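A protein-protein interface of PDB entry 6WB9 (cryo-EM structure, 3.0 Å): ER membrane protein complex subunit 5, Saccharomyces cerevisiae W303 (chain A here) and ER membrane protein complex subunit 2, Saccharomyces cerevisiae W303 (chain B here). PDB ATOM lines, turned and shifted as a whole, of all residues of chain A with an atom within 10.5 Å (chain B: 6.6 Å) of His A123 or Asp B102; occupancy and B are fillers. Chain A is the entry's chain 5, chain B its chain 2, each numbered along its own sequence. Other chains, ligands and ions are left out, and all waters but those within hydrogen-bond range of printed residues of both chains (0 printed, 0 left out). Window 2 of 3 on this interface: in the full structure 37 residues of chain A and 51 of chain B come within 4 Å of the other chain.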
ATOM      1  N   SER A 118     -18.876  23.972  -3.712  1.00  0.00           N
ATOM      2  CA  SER A 118     -19.086  22.960  -4.734  1.00  0.00           C
ATOM      3  C   SER A 118     -18.637  21.586  -4.273  1.00  0.00           C
ATOM      4  O   SER A 118     -19.266  20.583  -4.627  1.00  0.00           O
ATOM      5  CB  SER A 118     -18.341  23.340  -6.015  1.00  0.00           C
ATOM      6  OG  SER A 118     -18.733  24.620  -6.474  1.00  0.00           O
ATOM      7  N   PHE A 119     -17.566  21.525  -3.493  1.00  0.00           N
ATOM      8  CA  PHE A 119     -17.021  20.274  -2.971  1.00  0.00           C
ATOM      9  C   PHE A 119     -17.539  19.978  -1.573  1.00  0.00           C
ATOM     10  O   PHE A 119     -16.767  19.738  -0.649  1.00  0.00           O
ATOM     11  CB  PHE A 119     -15.503  20.331  -2.975  1.00  0.00           C
ATOM     12  CG  PHE A 119     -14.920  20.709  -4.294  1.00  0.00           C
ATOM     13  CD1 PHE A 119     -14.766  19.761  -5.288  1.00  0.00           C
ATOM     14  CD2 PHE A 119     -14.518  22.010  -4.540  1.00  0.00           C
ATOM     15  CE1 PHE A 119     -14.226  20.106  -6.502  1.00  0.00           C
ATOM     16  CE2 PHE A 119     -13.981  22.358  -5.754  1.00  0.00           C
ATOM     17  CZ  PHE A 119     -13.829  21.403  -6.730  1.00  0.00           C
ATOM     18  N   VAL A 120     -18.853  19.990  -1.392  1.00  0.00           N
ATOM     19  CA  VAL A 120     -19.451  19.628  -0.114  1.00  0.00           C
ATOM     20  C   VAL A 120     -19.770  18.143  -0.160  1.00  0.00           C
ATOM     21  O   VAL A 120     -20.520  17.689  -1.031  1.00  0.00           O
ATOM     22  CB  VAL A 120     -20.714  20.450   0.174  1.00  0.00           C
ATOM     23  CG1 VAL A 120     -21.381  19.966   1.450  1.00  0.00           C
ATOM     24  CG2 VAL A 120     -20.384  21.914   0.265  1.00  0.00           C
ATOM     25  N   ASP A 121     -19.192  17.384   0.762  1.00  0.00           N
ATOM     26  CA  ASP A 121     -19.582  15.991   0.932  1.00  0.00           C
ATOM     27  C   ASP A 121     -20.980  15.983   1.531  1.00  0.00           C
ATOM     28  O   ASP A 121     -21.157  16.232   2.725  1.00  0.00           O
ATOM     29  CB  ASP A 121     -18.584  15.249   1.811  1.00  0.00           C
ATOM     30  CG  ASP A 121     -17.215  15.139   1.171  1.00  0.00           C
ATOM     31  OD1 ASP A 121     -17.128  15.229  -0.073  1.00  0.00           O
ATOM     32  OD2 ASP A 121     -16.224  14.959   1.910  1.00  0.00           O
ATOM     33  N   VAL A 122     -21.977  15.724   0.680  1.00  0.00           N
ATOM     34  CA  VAL A 122     -23.377  15.824   1.079  1.00  0.00           C
ATOM     35  C   VAL A 122     -23.725  14.741   2.090  1.00  0.00           C
ATOM     36  O   VAL A 122     -24.441  14.992   3.070  1.00  0.00           O
ATOM     37  CB  VAL A 122     -24.277  15.757  -0.168  1.00  0.00           C
ATOM     38  CG1 VAL A 122     -25.734  15.882   0.207  1.00  0.00           C
ATOM     39  CG2 VAL A 122     -23.890  16.844  -1.154  1.00  0.00           C
ATOM     40  N   HIS A 123     -23.193  13.531   1.891  1.00  0.00           N
ATOM     41  CA  HIS A 123     -23.426  12.442   2.833  1.00  0.00           C
ATOM     42  C   HIS A 123     -22.773  12.710   4.182  1.00  0.00           C
ATOM     43  O   HIS A 123     -23.306  12.294   5.212  1.00  0.00           O
ATOM     44  CB  HIS A 123     -22.915  11.127   2.251  1.00  0.00           C
ATOM     45  CG  HIS A 123     -23.546  10.762   0.945  1.00  0.00           C
ATOM     46  ND1 HIS A 123     -24.892  10.501   0.818  1.00  0.00           N
ATOM     47  CD2 HIS A 123     -23.015  10.614  -0.292  1.00  0.00           C
ATOM     48  CE1 HIS A 123     -25.164  10.208  -0.441  1.00  0.00           C
ATOM     49  NE2 HIS A 123     -24.042  10.270  -1.135  1.00  0.00           N
ATOM     50  N   MET A 124     -21.650  13.434   4.200  1.00  0.00           N
ATOM     51  CA  MET A 124     -21.022  13.789   5.469  1.00  0.00           C
ATOM     52  C   MET A 124     -21.855  14.810   6.235  1.00  0.00           C
ATOM     53  O   MET A 124     -21.995  14.706   7.458  1.00  0.00           O
ATOM     54  CB  MET A 124     -19.611  14.323   5.226  1.00  0.00           C
ATOM     55  CG  MET A 124     -18.819  14.591   6.491  1.00  0.00           C
ATOM     56  SD  MET A 124     -18.605  13.113   7.500  1.00  0.00           S
ATOM     57  CE  MET A 124     -17.621  13.761   8.848  1.00  0.00           C
ATOM     58  N   LYS A 125     -22.426  15.794   5.529  1.00  0.00           N
ATOM     59  CA  LYS A 125     -23.309  16.767   6.169  1.00  0.00           C
ATOM     60  C   LYS A 125     -24.574  16.100   6.695  1.00  0.00           C
ATOM     61  O   LYS A 125     -25.028  16.407   7.806  1.00  0.00           O
ATOM     62  CB  LYS A 125     -23.669  17.880   5.186  1.00  0.00           C
ATOM     63  CG  LYS A 125     -22.481  18.617   4.596  1.00  0.00           C
ATOM     64  CD  LYS A 125     -21.959  19.688   5.530  1.00  0.00           C
ATOM     65  CE  LYS A 125     -22.933  20.843   5.634  1.00  0.00           C
ATOM     66  NZ  LYS A 125     -22.394  21.934   6.485  1.00  0.00           N
ATOM     67  N   ARG A 126     -25.139  15.170   5.918  1.00  0.00           N
ATOM     68  CA  ARG A 126     -26.319  14.439   6.366  1.00  0.00           C
ATOM     69  C   ARG A 126     -25.997  13.527   7.545  1.00  0.00           C
ATOM     70  O   ARG A 126     -26.816  13.380   8.456  1.00  0.00           O
ATOM     71  CB  ARG A 126     -26.908  13.634   5.212  1.00  0.00           C
ATOM     72  CG  ARG A 126     -27.491  14.488   4.108  1.00  0.00           C
ATOM     73  CD  ARG A 126     -27.994  13.638   2.963  1.00  0.00           C
ATOM     74  NE  ARG A 126     -29.155  12.844   3.348  1.00  0.00           N
ATOM     75  CZ  ARG A 126     -30.412  13.253   3.218  1.00  0.00           C
ATOM     76  NH1 ARG A 126     -30.671  14.448   2.711  1.00  0.00           N
ATOM     77  NH2 ARG A 126     -31.409  12.466   3.594  1.00  0.00           N
ATOM     78  N   LYS A 127     -24.796  12.941   7.561  1.00  0.00           N
ATOM     79  CA  LYS A 127     -24.375  12.104   8.680  1.00  0.00           C
ATOM     80  C   LYS A 127     -24.194  12.922   9.951  1.00  0.00           C
ATOM     81  O   LYS A 127     -24.624  12.496  11.029  1.00  0.00           O
ATOM     82  CB  LYS A 127     -23.076  11.381   8.325  1.00  0.00           C
ATOM     83  CG  LYS A 127     -22.519  10.493   9.426  1.00  0.00           C
ATOM     84  CD  LYS A 127     -21.042  10.200   9.204  1.00  0.00           C
ATOM     85  CE  LYS A 127     -20.788   9.598   7.830  1.00  0.00           C
ATOM     86  NZ  LYS A 127     -19.334   9.409   7.566  1.00  0.00           N
ATOM     87  N   ILE A 128     -23.578  14.102   9.839  1.00  0.00           N
ATOM     88  CA  ILE A 128     -23.365  14.955  11.006  1.00  0.00           C
ATOM     89  C   ILE A 128     -24.694  15.487  11.538  1.00  0.00           C
ATOM     90  O   ILE A 128     -24.927  15.500  12.754  1.00  0.00           O
ATOM     91  CB  ILE A 128     -22.379  16.087  10.656  1.00  0.00           C
ATOM     92  CG1 ILE A 128     -20.977  15.517  10.443  1.00  0.00           C
ATOM     93  CG2 ILE A 128     -22.315  17.132  11.753  1.00  0.00           C
ATOM     94  CD1 ILE A 128     -19.965  16.542   9.984  1.00  0.00           C
ATOM     95  N   CYS A 129     -25.614  15.861  10.640  1.00  0.00           N
ATOM     96  CA  CYS A 129     -26.916  16.352  11.087  1.00  0.00           C
ATOM     97  C   CYS A 129     -27.772  15.234  11.674  1.00  0.00           C
ATOM     98  O   CYS A 129     -28.506  15.456  12.644  1.00  0.00           O
ATOM     99  CB  CYS A 129     -27.642  17.037   9.932  1.00  0.00           C
ATOM    100  SG  CYS A 129     -26.937  18.633   9.462  1.00  0.00           S
ATOM    101  N   ARG A 130     -27.666  14.018  11.127  1.00  0.00           N
ATOM    102  CA  ARG A 130     -28.416  12.889  11.668  1.00  0.00           C
ATOM    103  C   ARG A 130     -27.876  12.466  13.029  1.00  0.00           C
ATOM    104  O   ARG A 130     -28.650  12.131  13.931  1.00  0.00           O
ATOM    105  CB  ARG A 130     -28.373  11.721  10.685  1.00  0.00           C
ATOM    106  CG  ARG A 130     -29.436  10.666  10.920  1.00  0.00           C
ATOM    107  CD  ARG A 130     -29.233   9.443  10.031  1.00  0.00           C
ATOM    108  NE  ARG A 130     -29.250   9.762   8.604  1.00  0.00           N
ATOM    109  CZ  ARG A 130     -28.187   9.694   7.809  1.00  0.00           C
ATOM    110  NH1 ARG A 130     -27.014   9.316   8.298  1.00  0.00           N
ATOM    111  NH2 ARG A 130     -28.295  10.003   6.523  1.00  0.00           N
ATOM    112  N   GLU A 131     -26.551  12.488  13.199  1.00  0.00           N
ATOM    113  CA  GLU A 131     -25.968  12.162  14.495  1.00  0.00           C
ATOM    114  C   GLU A 131     -26.207  13.267  15.516  1.00  0.00           C
ATOM    115  O   GLU A 131     -26.220  12.999  16.722  1.00  0.00           O
ATOM    116  CB  GLU A 131     -24.472  11.888  14.344  1.00  0.00           C
ATOM    117  CG  GLU A 131     -24.154  10.568  13.660  1.00  0.00           C
ATOM    118  CD  GLU A 131     -22.693  10.447  13.278  1.00  0.00           C
ATOM    119  OE1 GLU A 131     -21.937  11.415  13.501  1.00  0.00           O
ATOM    120  OE2 GLU A 131     -22.300   9.384  12.752  1.00  0.00           O
ATOM    121  N   LEU B  96     -30.515  12.921  -6.829  1.00  0.00           N
ATOM    122  CA  LEU B  96     -30.106  11.575  -7.211  1.00  0.00           C
ATOM    123  C   LEU B  96     -29.131  10.995  -6.197  1.00  0.00           C
ATOM    124  O   LEU B  96     -29.148   9.791  -5.935  1.00  0.00           O
ATOM    125  CB  LEU B  96     -29.473  11.584  -8.601  1.00  0.00           C
ATOM    126  CG  LEU B  96     -30.389  11.744  -9.811  1.00  0.00           C
ATOM    127  CD1 LEU B  96     -29.565  11.807 -11.086  1.00  0.00           C
ATOM    128  CD2 LEU B  96     -31.389  10.605  -9.872  1.00  0.00           C
ATOM    129  N   GLN B  97     -28.285  11.842  -5.609  1.00  0.00           N
ATOM    130  CA  GLN B  97     -27.229  11.363  -4.726  1.00  0.00           C
ATOM    131  C   GLN B  97     -27.770  10.930  -3.369  1.00  0.00           C
ATOM    132  O   GLN B  97     -27.256   9.980  -2.768  1.00  0.00           O
ATOM    133  CB  GLN B  97     -26.174  12.456  -4.562  1.00  0.00           C
ATOM    134  CG  GLN B  97     -24.871  12.002  -3.946  1.00  0.00           C
ATOM    135  CD  GLN B  97     -23.852  13.116  -3.886  1.00  0.00           C
ATOM    136  OE1 GLN B  97     -24.121  14.240  -4.308  1.00  0.00           O
ATOM    137  NE2 GLN B  97     -22.673  12.812  -3.360  1.00  0.00           N
ATOM    138  N   ILE B  98     -28.800  11.607  -2.861  1.00  0.00           N
ATOM    139  CA  ILE B  98     -29.303  11.267  -1.535  1.00  0.00           C
ATOM    140  C   ILE B  98     -30.330  10.138  -1.557  1.00  0.00           C
ATOM    141  O   ILE B  98     -30.580   9.523  -0.512  1.00  0.00           O
ATOM    142  CB  ILE B  98     -29.897  12.498  -0.827  1.00  0.00           C
ATOM    143  CG1 ILE B  98     -31.104  13.041  -1.592  1.00  0.00           C
ATOM    144  CG2 ILE B  98     -28.839  13.575  -0.670  1.00  0.00           C
ATOM    145  CD1 ILE B  98     -31.755  14.227  -0.924  1.00  0.00           C
ATOM    146  N   ASN B  99     -30.932   9.851  -2.706  1.00  0.00           N
ATOM    147  CA  ASN B  99     -31.856   8.724  -2.853  1.00  0.00           C
ATOM    148  C   ASN B  99     -31.140   7.491  -3.391  1.00  0.00           C
ATOM    149  O   ASN B  99     -31.559   6.902  -4.386  1.00  0.00           O
ATOM    150  CB  ASN B  99     -33.019   9.113  -3.757  1.00  0.00           C
ATOM    151  CG  ASN B  99     -33.731  10.363  -3.284  1.00  0.00           C
ATOM    152  OD1 ASN B  99     -33.769  10.658  -2.091  1.00  0.00           O
ATOM    153  ND2 ASN B  99     -34.302  11.108  -4.224  1.00  0.00           N
ATOM    154  N   GLY B 100     -30.061   7.075  -2.729  1.00  0.00           N
ATOM    155  CA  GLY B 100     -29.202   6.052  -3.307  1.00  0.00           C
ATOM    156  C   GLY B 100     -28.475   6.618  -4.511  1.00  0.00           C
ATOM    157  O   GLY B 100     -27.926   7.721  -4.452  1.00  0.00           O
ATOM    158  N   ASN B 101     -28.425   5.818  -5.587  1.00  0.00           N
ATOM    159  CA  ASN B 101     -28.235   6.259  -6.984  1.00  0.00           C
ATOM    160  C   ASN B 101     -27.018   7.162  -7.196  1.00  0.00           C
ATOM    161  O   ASN B 101     -27.069   8.130  -7.958  1.00  0.00           O
ATOM    162  CB  ASN B 101     -29.496   6.948  -7.507  1.00  0.00           C
ATOM    163  CG  ASN B 101     -30.715   6.054  -7.453  1.00  0.00           C
ATOM    164  OD1 ASN B 101     -30.792   5.138  -6.636  1.00  0.00           O
ATOM    165  ND2 ASN B 101     -31.678   6.316  -8.328  1.00  0.00           N
ATOM    166  N   ASP B 102     -25.923   6.861  -6.492  1.00  0.00           N
ATOM    167  CA  ASP B 102     -24.701   7.646  -6.655  1.00  0.00           C
ATOM    168  C   ASP B 102     -24.098   7.440  -8.039  1.00  0.00           C
ATOM    169  O   ASP B 102     -23.666   8.404  -8.688  1.00  0.00           O
ATOM    170  CB  ASP B 102     -23.687   7.277  -5.572  1.00  0.00           C
ATOM    171  CG  ASP B 102     -24.104   7.748  -4.194  1.00  0.00           C
ATOM    172  OD1 ASP B 102     -25.123   8.459  -4.089  1.00  0.00           O
ATOM    173  OD2 ASP B 102     -23.409   7.409  -3.215  1.00  0.00           O
ATOM    174  N   LYS B 103     -24.078   6.190  -8.510  1.00  0.00           N
ATOM    175  CA  LYS B 103     -23.623   5.908  -9.866  1.00  0.00           C
ATOM    176  C   LYS B 103     -24.573   6.483 -10.906  1.00  0.00           C
ATOM    177  O   LYS B 103     -24.135   6.850 -11.999  1.00  0.00           O
ATOM    178  CB  LYS B 103     -23.460   4.401 -10.062  1.00  0.00           C
ATOM    179  CG  LYS B 103     -22.323   3.794  -9.256  1.00  0.00           C
ATOM    180  CD  LYS B 103     -22.165   2.310  -9.544  1.00  0.00           C
ATOM    181  CE  LYS B 103     -20.911   1.748  -8.888  1.00  0.00           C
ATOM    182  NZ  LYS B 103     -20.916   1.929  -7.410  1.00  0.00           N
ATOM    183  N   GLY B 104     -25.862   6.598 -10.576  1.00  0.00           N
ATOM    184  CA  GLY B 104     -26.790   7.268 -11.473  1.00  0.00           C
ATOM    185  C   GLY B 104     -26.509   8.753 -11.599  1.00  0.00           C
ATOM    186  O   GLY B 104     -26.605   9.319 -12.692  1.00  0.00           O
ATOM    187  N   ALA B 105     -26.127   9.397 -10.492  1.00  0.00           N
ATOM    188  CA  ALA B 105     -25.747  10.807 -10.542  1.00  0.00           C
ATOM    189  C   ALA B 105     -24.438  10.999 -11.297  1.00  0.00           C
ATOM    190  O   ALA B 105     -24.278  11.984 -12.029  1.00  0.00           O
ATOM    191  CB  ALA B 105     -25.640  11.373  -9.128  1.00  0.00           C
ATOM    192  N   ILE B 106     -23.501  10.054 -11.142  1.00  0.00           N
ATOM    193  CA  ILE B 106     -22.252  10.094 -11.903  1.00  0.00           C
ATOM    194  C   ILE B 106     -22.525   9.939 -13.395  1.00  0.00           C
ATOM    195  O   ILE B 106     -21.968  10.677 -14.217  1.00  0.00           O
ATOM    196  CB  ILE B 106     -21.281   9.013 -11.385  1.00  0.00           C
ATOM    197  CG1 ILE B 106     -20.789   9.370  -9.985  1.00  0.00           C
ATOM    198  CG2 ILE B 106     -20.087   8.842 -12.314  1.00  0.00           C
ATOM    199  CD1 ILE B 106     -19.890   8.329  -9.369  1.00  0.00           C
ATOM    200  N   GLU B 107     -23.415   9.005 -13.761  1.00  0.00           N
ATOM    201  CA  GLU B 107     -23.791   8.808 -15.160  1.00  0.00           C
ATOM    202  C   GLU B 107     -24.483  10.038 -15.733  1.00  0.00           C
ATOM    203  O   GLU B 107     -24.205  10.436 -16.871  1.00  0.00           O
ATOM    204  CB  GLU B 107     -24.704   7.589 -15.294  1.00  0.00           C
ATOM    205  CG  GLU B 107     -24.001   6.245 -15.224  1.00  0.00           C
ATOM    206  CD  GLU B 107     -24.977   5.094 -15.046  1.00  0.00           C
ATOM    207  OE1 GLU B 107     -26.181   5.358 -14.843  1.00  0.00           O
ATOM    208  OE2 GLU B 107     -24.541   3.925 -15.108  1.00  0.00           O
ATOM    209  N   ILE B 136     -19.134  14.215  -6.208  1.00  0.00           N
ATOM    210  CA  ILE B 136     -19.843  12.938  -6.155  1.00  0.00           C
ATOM    211  C   ILE B 136     -18.867  11.773  -6.313  1.00  0.00           C
ATOM    212  O   ILE B 136     -19.014  10.732  -5.659  1.00  0.00           O
ATOM    213  CB  ILE B 136     -20.973  12.906  -7.204  1.00  0.00           C
ATOM    214  CG1 ILE B 136     -22.000  13.996  -6.906  1.00  0.00           C
ATOM    215  CG2 ILE B 136     -21.711  11.582  -7.183  1.00  0.00           C
ATOM    216  CD1 ILE B 136     -23.161  14.038  -7.876  1.00  0.00           C
ATOM    217  N   THR B 139     -17.336  11.371  -2.875  1.00  0.00           N
ATOM    218  CA  THR B 139     -18.200  10.762  -1.863  1.00  0.00           C
ATOM    219  C   THR B 139     -18.455   9.286  -2.153  1.00  0.00           C
ATOM    220  O   THR B 139     -18.328   8.438  -1.262  1.00  0.00           O
ATOM    221  CB  THR B 139     -19.526  11.515  -1.771  1.00  0.00           C
ATOM    222  OG1 THR B 139     -20.124  11.595  -3.071  1.00  0.00           O
ATOM    223  CG2 THR B 139     -19.310  12.913  -1.223  1.00  0.00           C
ATOM    224  N   SER B 140     -18.817   8.960  -3.395  1.00  0.00           N
ATOM    225  CA  SER B 140     -19.274   7.612  -3.726  1.00  0.00           C
ATOM    226  C   SER B 140     -18.120   6.621  -3.808  1.00  0.00           C
ATOM    227  O   SER B 140     -18.160   5.559  -3.178  1.00  0.00           O
ATOM    228  CB  SER B 140     -20.039   7.633  -5.048  1.00  0.00           C
ATOM    229  OG  SER B 140     -19.177   7.965  -6.121  1.00  0.00           O
ATOM    230  N   LYS B 141     -17.086   6.948  -4.583  1.00  0.00           N
ATOM    231  CA  LYS B 141     -15.995   6.013  -4.823  1.00  0.00           C
ATOM    232  C   LYS B 141     -15.027   5.896  -3.653  1.00  0.00           C
ATOM    233  O   LYS B 141     -14.161   5.014  -3.694  1.00  0.00           O
ATOM    234  CB  LYS B 141     -15.223   6.420  -6.079  1.00  0.00           C
ATOM    235  CG  LYS B 141     -16.063   6.465  -7.341  1.00  0.00           C
ATOM    236  CD  LYS B 141     -15.202   6.768  -8.553  1.00  0.00           C
ATOM    237  CE  LYS B 141     -16.028   6.800  -9.826  1.00  0.00           C
ATOM    238  NZ  LYS B 141     -15.176   7.006 -11.030  1.00  0.00           N
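The side-chain amide nitrogen of Gln B97 lies within hydrogen-bond range of the side-chain hydroxyl of Thr B139 (2.8 Å).
The backbone carbonyl oxygen of Ile B136 is in hydrogen-bond range of the side-chain hydroxyl of Thr B139, at 2.9 Å.
Among the printed residues, merely in contact across the chains: His A123 with Gln B97 (3.1 Å), Asp A121 with Thr B139 (3.4 Å), His A123 with Asp B102 (3.6 Å), Arg A126 with Ile B98 (3.7 Å), His A123 with Thr B139 (3.9 Å) and Val A122 with Ile B98 (3.97 Å).
Of the printed residues of chain B, His A123 touches Gln B97, Asp B102 and Thr B139.
Asp B102 touches just one residue of chain A: His A123.
Of chain A, only His A123 comes within 4 Å of Gln B97.
No residue of chain A comes within 4 Å of Gly B100.
Thr B139 touches two residues of chain A.
Of the printed residues of chain B, Asp A121 touches Thr B139 (3.4 Å).
Printed residues of chain B within 4 Å of Val A122: Ile B98 (3.97 Å).
Glu B107 touches none of the printed residues of chain A.
The nearest residue of chain B that does not touch His A123 is Ile B98 (4.4 Å).
Of the 16 printed residues of chain B, 4 touch a printed residue of chain A.
Hydrophobic or aromatic side chains of chain B that line the printed part of chain A: Ile B98.
Of the 14 printed residues of chain A, 4 touch a printed residue of chain B.
Hydrophobic or aromatic side chains of chain A within 4 Å of the printed part of chain B: Val A122 and His A123.
Among the printed residues, 6 pairs touch across the chains.
Among the printed residues, no Asp or Glu carboxylate lies within 4 Å of a Lys or Arg side-chain nitrogen of the other chain.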
